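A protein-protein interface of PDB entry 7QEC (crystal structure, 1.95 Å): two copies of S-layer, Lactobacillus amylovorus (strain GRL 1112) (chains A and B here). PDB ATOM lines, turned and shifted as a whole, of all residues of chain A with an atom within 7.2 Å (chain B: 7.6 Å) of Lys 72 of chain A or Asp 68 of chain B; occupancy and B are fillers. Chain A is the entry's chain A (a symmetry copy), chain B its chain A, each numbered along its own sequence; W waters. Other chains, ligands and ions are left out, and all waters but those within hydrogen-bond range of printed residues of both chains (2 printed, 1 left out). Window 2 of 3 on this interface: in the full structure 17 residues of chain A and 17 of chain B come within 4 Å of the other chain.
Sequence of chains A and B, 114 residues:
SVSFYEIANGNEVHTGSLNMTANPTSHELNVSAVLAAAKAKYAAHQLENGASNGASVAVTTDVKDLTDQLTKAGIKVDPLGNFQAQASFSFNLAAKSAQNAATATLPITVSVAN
O of Lys 72 of chain A lies within hydrogen-bond range of NE2 of Gln 69 of chain B (3.4 Å). The side-chain amide nitrogen of Gln 69 of chain A lies within hydrogen-bond range of the backbone carbonyl oxygen of Lys 72 of chain B (3.4 Å).
The backbone NH of Asp 65 of chain B lies within hydrogen-bond range of the side-chain carboxylate of Asp 62 of chain B (3.0 Å). The backbone NH (N) of Ala 94 of chain B sits at hydrogen-bond distance from the side-chain hydroxyl (OG1) of Thr 61 of chain B (2.9 Å). The side-chain amide oxygen of Gln 69 of chain B sits at hydrogen-bond distance from the backbone NH of Asn 92 of chain B.
Among the printed residues, merely in contact across the chains: Asp 68 of chain A with Lys 72 of chain B (3.3 Å), Gln 69 of chain A with Gln 69 of chain B (3.99 Å), Gln 69 of chain A with Ala 73 of chain B (3.8 Å), Lys 72 of chain A with Asp 65 of chain B (3.9 Å), Lys 72 of chain A with Asp 68 of chain B (3.3 Å), Ala 73 of chain A with Gln 69 of chain B (3.8 Å), Ala 73 of chain A with Asn 92 of chain B (3.7 Å) and Ala 73 of chain A with Ala 94 of chain B (3.5 Å).
Leu 66 of chain A touches none of the printed residues of chain B. Of the printed residues of chain B, Asp 68 of chain A touches Lys 72. Lys 72 of chain A touches just these residues of chain B: Asp 65, Asp 68 and Gln 69. Asp 62 of chain B touches none of the printed residues of chain A. Printed residues of chain A within 4 Å of Asp 65 of chain B: Lys 72 (3.9 Å). Asp 68 of chain B touches just one residue of chain A: Lys 72 (3.3 Å). Printed residues of chain A within 4 Å of Gln 69 of chain B: Gln 69, Lys 72 and Ala 73. Of the printed residues of chain A, Ala 73 of chain B touches Gln 69. Of the printed residues of chain A, Ala 94 of chain B touches Ala 73 (3.5 Å). The nearest residue of chain B that does not touch Lys 72 of chain A is Lys 72 of chain B (4.5 Å).
Of the 19 printed residues of chain B, 7 touch a printed residue of chain A. Printed residues of chain B that touch a printed residue of chain A: Asp 65, Asp 68, Gln 69, Lys 72, Ala 73, Asn 92 and Ala 94. Of the 10 printed residues of chain A, 4 touch a printed residue of chain B. Hydrophobic or aromatic side chains of chain A that line the printed part of chain B: Ala 73.
Asp 68 of chain A touches Lys 72 of chain B, and with the chains exchanged Lys 72 of chain A touches Asp 68 of chain B. Gln 69 of chain A touches its own counterpart, Gln 69 of chain B. Gln 69 of chain A touches Lys 72 of chain B, and with the chains exchanged Lys 72 of chain A touches Gln 69 of chain B. Gln 69 of chain A touches Ala 73 of chain B, and with the chains exchanged Ala 73 of chain A touches Gln 69 of chain B. Positions printed for both chains: 66, 67, 68, 69, 70, 71, 72, 73, 74 and 75.
Water W1 lies within hydrogen-bond range of OG1 of Thr 61 of chain B (2.8 Å) and O of Lys 72 of chain A (3.2 Å). Water W2 bridges the side-chain amide oxygen of Gln 69 of chain B (3.5 Å) and the side-chain amide oxygen of Gln 69 of chain A (3.5 Å).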
ATOM      1  N   LEU A  66     -24.483  11.880  -4.070  1.00  0.00           N
ATOM      2  CA  LEU A  66     -23.065  11.963  -4.392  1.00  0.00           C
ATOM      3  C   LEU A  66     -22.231  12.174  -3.135  1.00  0.00           C
ATOM      4  O   LEU A  66     -21.149  11.591  -2.997  1.00  0.00           O
ATOM      5  CB  LEU A  66     -22.822  13.085  -5.401  1.00  0.00           C
ATOM      6  CG  LEU A  66     -21.362  13.286  -5.813  1.00  0.00           C
ATOM      7  CD1 LEU A  66     -20.744  11.952  -6.239  1.00  0.00           C
ATOM      8  CD2 LEU A  66     -21.270  14.318  -6.938  1.00  0.00           C
ATOM      9  N   THR A  67     -22.730  12.982  -2.194  1.00  0.00           N
ATOM     10  CA  THR A  67     -22.011  13.164  -0.934  1.00  0.00           C
ATOM     11  C   THR A  67     -21.851  11.832  -0.194  1.00  0.00           C
ATOM     12  O   THR A  67     -20.767  11.523   0.318  1.00  0.00           O
ATOM     13  CB  THR A  67     -22.731  14.201  -0.055  1.00  0.00           C
ATOM     14  OG1 THR A  67     -22.763  15.463  -0.728  1.00  0.00           O
ATOM     15  CG2 THR A  67     -21.998  14.390   1.269  1.00  0.00           C
ATOM     16  N   ASP A  68     -22.915  11.022  -0.149  1.00  0.00           N
ATOM     17  CA  ASP A  68     -22.857   9.732   0.542  1.00  0.00           C
ATOM     18  C   ASP A  68     -21.944   8.734  -0.175  1.00  0.00           C
ATOM     19  O   ASP A  68     -21.243   7.952   0.481  1.00  0.00           O
ATOM     20  CB  ASP A  68     -24.264   9.156   0.687  1.00  0.00           C
ATOM     21  CG  ASP A  68     -25.149   9.992   1.599  1.00  0.00           C
ATOM     22  OD1 ASP A  68     -24.599  10.750   2.425  1.00  0.00           O
ATOM     23  OD2 ASP A  68     -26.392   9.881   1.505  1.00  0.00           O
ATOM     24  N   GLN A  69     -21.950   8.723  -1.515  1.00  0.00           N
ATOM     25  CA  GLN A  69     -21.014   7.873  -2.252  1.00  0.00           C
ATOM     26  C   GLN A  69     -19.572   8.200  -1.878  1.00  0.00           C
ATOM     27  O   GLN A  69     -18.772   7.301  -1.588  1.00  0.00           O
ATOM     28  CB  GLN A  69     -21.203   8.035  -3.769  1.00  0.00           C
ATOM     29  CG  GLN A  69     -22.403   7.328  -4.385  1.00  0.00           C
ATOM     30  CD  GLN A  69     -22.442   7.477  -5.907  1.00  0.00           C
ATOM     31  OE1 GLN A  69     -21.485   7.130  -6.588  1.00  0.00           O
ATOM     32  NE2 GLN A  69     -23.540   7.996  -6.434  1.00  0.00           N
ATOM     33  N   LEU A  70     -19.212   9.490  -1.892  1.00  0.00           N
ATOM     34  CA  LEU A  70     -17.832   9.873  -1.598  1.00  0.00           C
ATOM     35  C   LEU A  70     -17.460   9.578  -0.146  1.00  0.00           C
ATOM     36  O   LEU A  70     -16.345   9.112   0.133  1.00  0.00           O
ATOM     37  CB  LEU A  70     -17.615  11.357  -1.919  1.00  0.00           C
ATOM     38  CG  LEU A  70     -17.905  11.782  -3.362  1.00  0.00           C
ATOM     39  CD1 LEU A  70     -17.800  13.299  -3.499  1.00  0.00           C
ATOM     40  CD2 LEU A  70     -16.972  11.090  -4.348  1.00  0.00           C
ATOM     41  N   THR A  71     -18.376   9.847   0.789  1.00  0.00           N
ATOM     42  CA  THR A  71     -18.119   9.571   2.203  1.00  0.00           C
ATOM     43  C   THR A  71     -17.793   8.097   2.444  1.00  0.00           C
ATOM     44  O   THR A  71     -16.932   7.767   3.270  1.00  0.00           O
ATOM     45  CB  THR A  71     -19.328   9.984   3.047  1.00  0.00           C
ATOM     46  OG1 THR A  71     -19.469  11.412   3.030  1.00  0.00           O
ATOM     47  CG2 THR A  71     -19.162   9.498   4.488  1.00  0.00           C
ATOM     48  N   LYS A  72     -18.470   7.194   1.736  1.00  0.00           N
ATOM     49  CA  LYS A  72     -18.220   5.764   1.894  1.00  0.00           C
ATOM     50  C   LYS A  72     -16.966   5.300   1.173  1.00  0.00           C
ATOM     51  O   LYS A  72     -16.562   4.148   1.345  1.00  0.00           O
ATOM     52  CB  LYS A  72     -19.430   4.970   1.398  1.00  0.00           C
ATOM     53  CG  LYS A  72     -20.646   5.183   2.247  1.00  0.00           C
ATOM     54  CD  LYS A  72     -20.302   4.885   3.706  1.00  0.00           C
ATOM     55  CE  LYS A  72     -21.539   4.862   4.586  1.00  0.00           C
ATOM     56  NZ  LYS A  72     -22.388   6.057   4.373  1.00  0.00           N
ATOM     57  N   ALA A  73     -16.352   6.156   0.365  1.00  0.00           N
ATOM     58  CA  ALA A  73     -15.068   5.875  -0.256  1.00  0.00           C
ATOM     59  C   ALA A  73     -13.888   6.397   0.562  1.00  0.00           C
ATOM     60  O   ALA A  73     -12.764   6.420   0.053  1.00  0.00           O
ATOM     61  CB  ALA A  73     -15.019   6.483  -1.660  1.00  0.00           C
ATOM     62  N   GLY A  74     -14.119   6.833   1.802  1.00  0.00           N
ATOM     63  CA  GLY A  74     -13.061   7.370   2.633  1.00  0.00           C
ATOM     64  C   GLY A  74     -12.767   8.852   2.468  1.00  0.00           C
ATOM     65  O   GLY A  74     -11.832   9.347   3.109  1.00  0.00           O
ATOM     66  N   ILE A  75     -13.528   9.575   1.642  1.00  0.00           N
ATOM     67  CA  ILE A  75     -13.300  11.000   1.388  1.00  0.00           C
ATOM     68  C   ILE A  75     -14.147  11.830   2.351  1.00  0.00           C
ATOM     69  O   ILE A  75     -15.349  11.586   2.500  1.00  0.00           O
ATOM     70  CB  ILE A  75     -13.636  11.350  -0.073  1.00  0.00           C
ATOM     71  CG1 ILE A  75     -12.761  10.532  -1.029  1.00  0.00           C
ATOM     72  CG2 ILE A  75     -13.487  12.858  -0.318  1.00  0.00           C
ATOM     73  CD1 ILE A  75     -12.986  10.824  -2.505  1.00  0.00           C
ATOM     74  N   VAL B  31     -21.309  -8.767  -3.553  1.00  0.00           N
ATOM     75  CA  VAL B  31     -20.399  -7.660  -3.241  1.00  0.00           C
ATOM     76  C   VAL B  31     -19.036  -8.178  -2.786  1.00  0.00           C
ATOM     77  O   VAL B  31     -17.991  -7.573  -3.080  1.00  0.00           O
ATOM     78  CB  VAL B  31     -21.038  -6.741  -2.177  1.00  0.00           C
ATOM     79  CG1 VAL B  31     -20.071  -5.673  -1.737  1.00  0.00           C
ATOM     80  CG2 VAL B  31     -22.290  -6.075  -2.723  1.00  0.00           C
ATOM     81  N   THR B  61     -10.827  -0.380   2.576  1.00  0.00           N
ATOM     82  CA  THR B  61     -12.201  -0.672   2.149  1.00  0.00           C
ATOM     83  C   THR B  61     -12.626  -2.101   2.516  1.00  0.00           C
ATOM     84  O   THR B  61     -11.975  -3.068   2.112  1.00  0.00           O
ATOM     85  CB  THR B  61     -12.316  -0.491   0.630  1.00  0.00           C
ATOM     86  OG1 THR B  61     -11.888   0.823   0.260  1.00  0.00           O
ATOM     87  CG2 THR B  61     -13.773  -0.704   0.141  1.00  0.00           C
ATOM     88  N   ASP B  62     -13.745  -2.242   3.241  1.00  0.00           N
ATOM     89  CA  ASP B  62     -14.278  -3.565   3.571  1.00  0.00           C
ATOM     90  C   ASP B  62     -15.643  -3.780   2.902  1.00  0.00           C
ATOM     91  O   ASP B  62     -16.138  -2.934   2.147  1.00  0.00           O
ATOM     92  CB  ASP B  62     -14.341  -3.775   5.095  1.00  0.00           C
ATOM     93  CG  ASP B  62     -15.382  -2.886   5.797  1.00  0.00           C
ATOM     94  OD1 ASP B  62     -16.175  -2.183   5.131  1.00  0.00           O
ATOM     95  OD2 ASP B  62     -15.407  -2.903   7.050  1.00  0.00           O
ATOM     96  N   VAL B  63     -16.263  -4.934   3.180  1.00  0.00           N
ATOM     97  CA  VAL B  63     -17.437  -5.310   2.383  1.00  0.00           C
ATOM     98  C   VAL B  63     -18.633  -4.407   2.697  1.00  0.00           C
ATOM     99  O   VAL B  63     -19.462  -4.132   1.819  1.00  0.00           O
ATOM    100  CB  VAL B  63     -17.756  -6.815   2.560  1.00  0.00           C
ATOM    101  CG1 VAL B  63     -18.499  -7.096   3.848  1.00  0.00           C
ATOM    102  CG2 VAL B  63     -18.531  -7.340   1.372  1.00  0.00           C
ATOM    103  N   LYS B  64     -18.733  -3.888   3.918  1.00  0.00           N
ATOM    104  CA  LYS B  64     -19.847  -2.981   4.172  1.00  0.00           C
ATOM    105  C   LYS B  64     -19.623  -1.591   3.568  1.00  0.00           C
ATOM    106  O   LYS B  64     -20.599  -0.934   3.190  1.00  0.00           O
ATOM    107  CB  LYS B  64     -20.128  -2.891   5.674  1.00  0.00           C
ATOM    108  CG  LYS B  64     -20.413  -4.245   6.327  1.00  0.00           C
ATOM    109  CD  LYS B  64     -21.828  -4.767   5.992  1.00  0.00           C
ATOM    110  CE  LYS B  64     -21.789  -6.022   5.099  1.00  0.00           C
ATOM    111  NZ  LYS B  64     -23.041  -6.236   4.315  1.00  0.00           N
ATOM    112  N   ASP B  65     -18.370  -1.124   3.458  1.00  0.00           N
ATOM    113  CA  ASP B  65     -18.109   0.137   2.755  1.00  0.00           C
ATOM    114  C   ASP B  65     -18.538   0.043   1.299  1.00  0.00           C
ATOM    115  O   ASP B  65     -19.194   0.952   0.767  1.00  0.00           O
ATOM    116  CB  ASP B  65     -16.622   0.511   2.823  1.00  0.00           C
ATOM    117  CG  ASP B  65     -16.142   0.805   4.238  1.00  0.00           C
ATOM    118  OD1 ASP B  65     -16.900   1.425   5.009  1.00  0.00           O
ATOM    119  OD2 ASP B  65     -14.990   0.423   4.574  1.00  0.00           O
ATOM    120  N   LEU B  66     -18.154  -1.047   0.631  1.00  0.00           N
ATOM    121  CA  LEU B  66     -18.533  -1.244  -0.762  1.00  0.00           C
ATOM    122  C   LEU B  66     -20.043  -1.381  -0.904  1.00  0.00           C
ATOM    123  O   LEU B  66     -20.633  -0.852  -1.853  1.00  0.00           O
ATOM    124  CB  LEU B  66     -17.820  -2.472  -1.328  1.00  0.00           C
ATOM    125  CG  LEU B  66     -18.145  -2.798  -2.788  1.00  0.00           C
ATOM    126  CD1 LEU B  66     -17.976  -1.550  -3.659  1.00  0.00           C
ATOM    127  CD2 LEU B  66     -17.254  -3.938  -3.284  1.00  0.00           C
ATOM    128  N   THR B  67     -20.691  -2.063   0.046  1.00  0.00           N
ATOM    129  CA  THR B  67     -22.149  -2.163   0.005  1.00  0.00           C
ATOM    130  C   THR B  67     -22.799  -0.778   0.072  1.00  0.00           C
ATOM    131  O   THR B  67     -23.736  -0.485  -0.682  1.00  0.00           O
ATOM    132  CB  THR B  67     -22.654  -3.066   1.145  1.00  0.00           C
ATOM    133  OG1 THR B  67     -22.118  -4.383   0.987  1.00  0.00           O
ATOM    134  CG2 THR B  67     -24.175  -3.168   1.120  1.00  0.00           C
ATOM    135  N   ASP B  68     -22.298   0.094   0.955  1.00  0.00           N
ATOM    136  CA  ASP B  68     -22.859   1.439   1.094  1.00  0.00           C
ATOM    137  C   ASP B  68     -22.590   2.307  -0.138  1.00  0.00           C
ATOM    138  O   ASP B  68     -23.449   3.107  -0.533  1.00  0.00           O
ATOM    139  CB  ASP B  68     -22.301   2.108   2.349  1.00  0.00           C
ATOM    140  CG  ASP B  68     -22.746   1.419   3.629  1.00  0.00           C
ATOM    141  OD1 ASP B  68     -23.776   0.714   3.594  1.00  0.00           O
ATOM    142  OD2 ASP B  68     -22.080   1.594   4.674  1.00  0.00           O
ATOM    143  N   GLN B  69     -21.402   2.188  -0.746  1.00  0.00           N
ATOM    144  CA  GLN B  69     -21.135   2.906  -1.994  1.00  0.00           C
ATOM    145  C   GLN B  69     -22.153   2.532  -3.066  1.00  0.00           C
ATOM    146  O   GLN B  69     -22.727   3.406  -3.727  1.00  0.00           O
ATOM    147  CB  GLN B  69     -19.716   2.608  -2.505  1.00  0.00           C
ATOM    148  CG  GLN B  69     -18.572   3.322  -1.795  1.00  0.00           C
ATOM    149  CD  GLN B  69     -17.218   3.028  -2.441  1.00  0.00           C
ATOM    150  OE1 GLN B  69     -17.039   3.251  -3.632  1.00  0.00           O
ATOM    151  NE2 GLN B  69     -16.273   2.526  -1.661  1.00  0.00           N
ATOM    152  N   LEU B  70     -22.384   1.228  -3.264  1.00  0.00           N
ATOM    153  CA  LEU B  70     -23.307   0.795  -4.313  1.00  0.00           C
ATOM    154  C   LEU B  70     -24.745   1.208  -4.006  1.00  0.00           C
ATOM    155  O   LEU B  70     -25.481   1.632  -4.910  1.00  0.00           O
ATOM    156  CB  LEU B  70     -23.211  -0.723  -4.507  1.00  0.00           C
ATOM    157  CG  LEU B  70     -21.826  -1.269  -4.870  1.00  0.00           C
ATOM    158  CD1 LEU B  70     -21.843  -2.796  -4.877  1.00  0.00           C
ATOM    159  CD2 LEU B  70     -21.346  -0.733  -6.212  1.00  0.00           C
ATOM    160  N   THR B  71     -25.163   1.085  -2.743  1.00  0.00           N
ATOM    161  CA  THR B  71     -26.515   1.482  -2.351  1.00  0.00           C
ATOM    162  C   THR B  71     -26.792   2.950  -2.672  1.00  0.00           C
ATOM    163  O   THR B  71     -27.903   3.308  -3.087  1.00  0.00           O
ATOM    164  CB  THR B  71     -26.725   1.224  -0.856  1.00  0.00           C
ATOM    165  OG1 THR B  71     -26.729  -0.188  -0.599  1.00  0.00           O
ATOM    166  CG2 THR B  71     -28.047   1.837  -0.391  1.00  0.00           C
ATOM    167  N   LYS B  72     -25.800   3.819  -2.485  1.00  0.00           N
ATOM    168  CA  LYS B  72     -25.971   5.239  -2.773  1.00  0.00           C
ATOM    169  C   LYS B  72     -25.888   5.557  -4.256  1.00  0.00           C
ATOM    170  O   LYS B  72     -26.159   6.694  -4.647  1.00  0.00           O
ATOM    171  CB  LYS B  72     -24.924   6.052  -2.008  1.00  0.00           C
ATOM    172  CG  LYS B  72     -25.124   5.994  -0.523  1.00  0.00           C
ATOM    173  CD  LYS B  72     -26.556   6.412  -0.189  1.00  0.00           C
ATOM    174  CE  LYS B  72     -26.758   6.594   1.304  1.00  0.00           C
ATOM    175  NZ  LYS B  72     -26.246   5.436   2.074  1.00  0.00           N
ATOM    176  N   ALA B  73     -25.509   4.591  -5.085  1.00  0.00           N
ATOM    177  CA  ALA B  73     -25.539   4.734  -6.531  1.00  0.00           C
ATOM    178  C   ALA B  73     -26.840   4.226  -7.149  1.00  0.00           C
ATOM    179  O   ALA B  73     -26.912   4.087  -8.374  1.00  0.00           O
ATOM    180  CB  ALA B  73     -24.356   3.991  -7.158  1.00  0.00           C
ATOM    181  N   GLY B  74     -27.854   3.927  -6.336  1.00  0.00           N
ATOM    182  CA  GLY B  74     -29.111   3.411  -6.839  1.00  0.00           C
ATOM    183  C   GLY B  74     -29.190   1.906  -7.030  1.00  0.00           C
ATOM    184  O   GLY B  74     -30.219   1.421  -7.516  1.00  0.00           O
ATOM    185  N   ILE B  75     -28.149   1.152  -6.665  1.00  0.00           N
ATOM    186  CA  ILE B  75     -28.114  -0.301  -6.844  1.00  0.00           C
ATOM    187  C   ILE B  75     -28.622  -0.983  -5.574  1.00  0.00           C
ATOM    188  O   ILE B  75     -28.181  -0.655  -4.467  1.00  0.00           O
ATOM    189  CB  ILE B  75     -26.687  -0.771  -7.181  1.00  0.00           C
ATOM    190  CG1 ILE B  75     -26.200  -0.104  -8.471  1.00  0.00           C
ATOM    191  CG2 ILE B  75     -26.629  -2.302  -7.279  1.00  0.00           C
ATOM    192  CD1 ILE B  75     -24.808  -0.524  -8.919  1.00  0.00           C
ATOM    193  N   VAL B  77     -28.970  -4.005  -2.976  1.00  0.00           N
ATOM    194  CA  VAL B  77     -28.187  -5.145  -2.487  1.00  0.00           C
ATOM    195  C   VAL B  77     -28.961  -5.821  -1.356  1.00  0.00           C
ATOM    196  O   VAL B  77     -29.260  -5.180  -0.339  1.00  0.00           O
ATOM    197  CB  VAL B  77     -26.790  -4.716  -1.998  1.00  0.00           C
ATOM    198  CG1 VAL B  77     -25.961  -5.948  -1.587  1.00  0.00           C
ATOM    199  CG2 VAL B  77     -26.049  -3.878  -3.060  1.00  0.00           C
ATOM    200  N   ASN B  92     -14.741   2.941  -5.509  1.00  0.00           N
ATOM    201  CA  ASN B  92     -13.408   3.395  -5.091  1.00  0.00           C
ATOM    202  C   ASN B  92     -12.811   2.480  -4.018  1.00  0.00           C
ATOM    203  O   ASN B  92     -13.485   2.130  -3.038  1.00  0.00           O
ATOM    204  CB  ASN B  92     -13.449   4.832  -4.547  1.00  0.00           C
ATOM    205  CG  ASN B  92     -13.932   5.860  -5.578  1.00  0.00           C
ATOM    206  OD1 ASN B  92     -15.035   6.392  -5.468  1.00  0.00           O
ATOM    207  ND2 ASN B  92     -13.102   6.159  -6.557  1.00  0.00           N
ATOM    208  N   ALA B  94      -9.962   2.499  -1.054  1.00  0.00           N
ATOM    209  CA  ALA B  94      -9.280   3.500  -0.236  1.00  0.00           C
ATOM    210  C   ALA B  94      -8.082   2.892   0.482  1.00  0.00           C
ATOM    211  O   ALA B  94      -8.087   1.720   0.862  1.00  0.00           O
ATOM    212  CB  ALA B  94     -10.230   4.129   0.797  1.00  0.00           C
HETATM  213  O   HOH W   1     -13.660   2.756   1.355  1.00  0.00           O
HETATM  214  O   HOH W   2     -18.701   5.128  -6.035  1.00  0.00           O
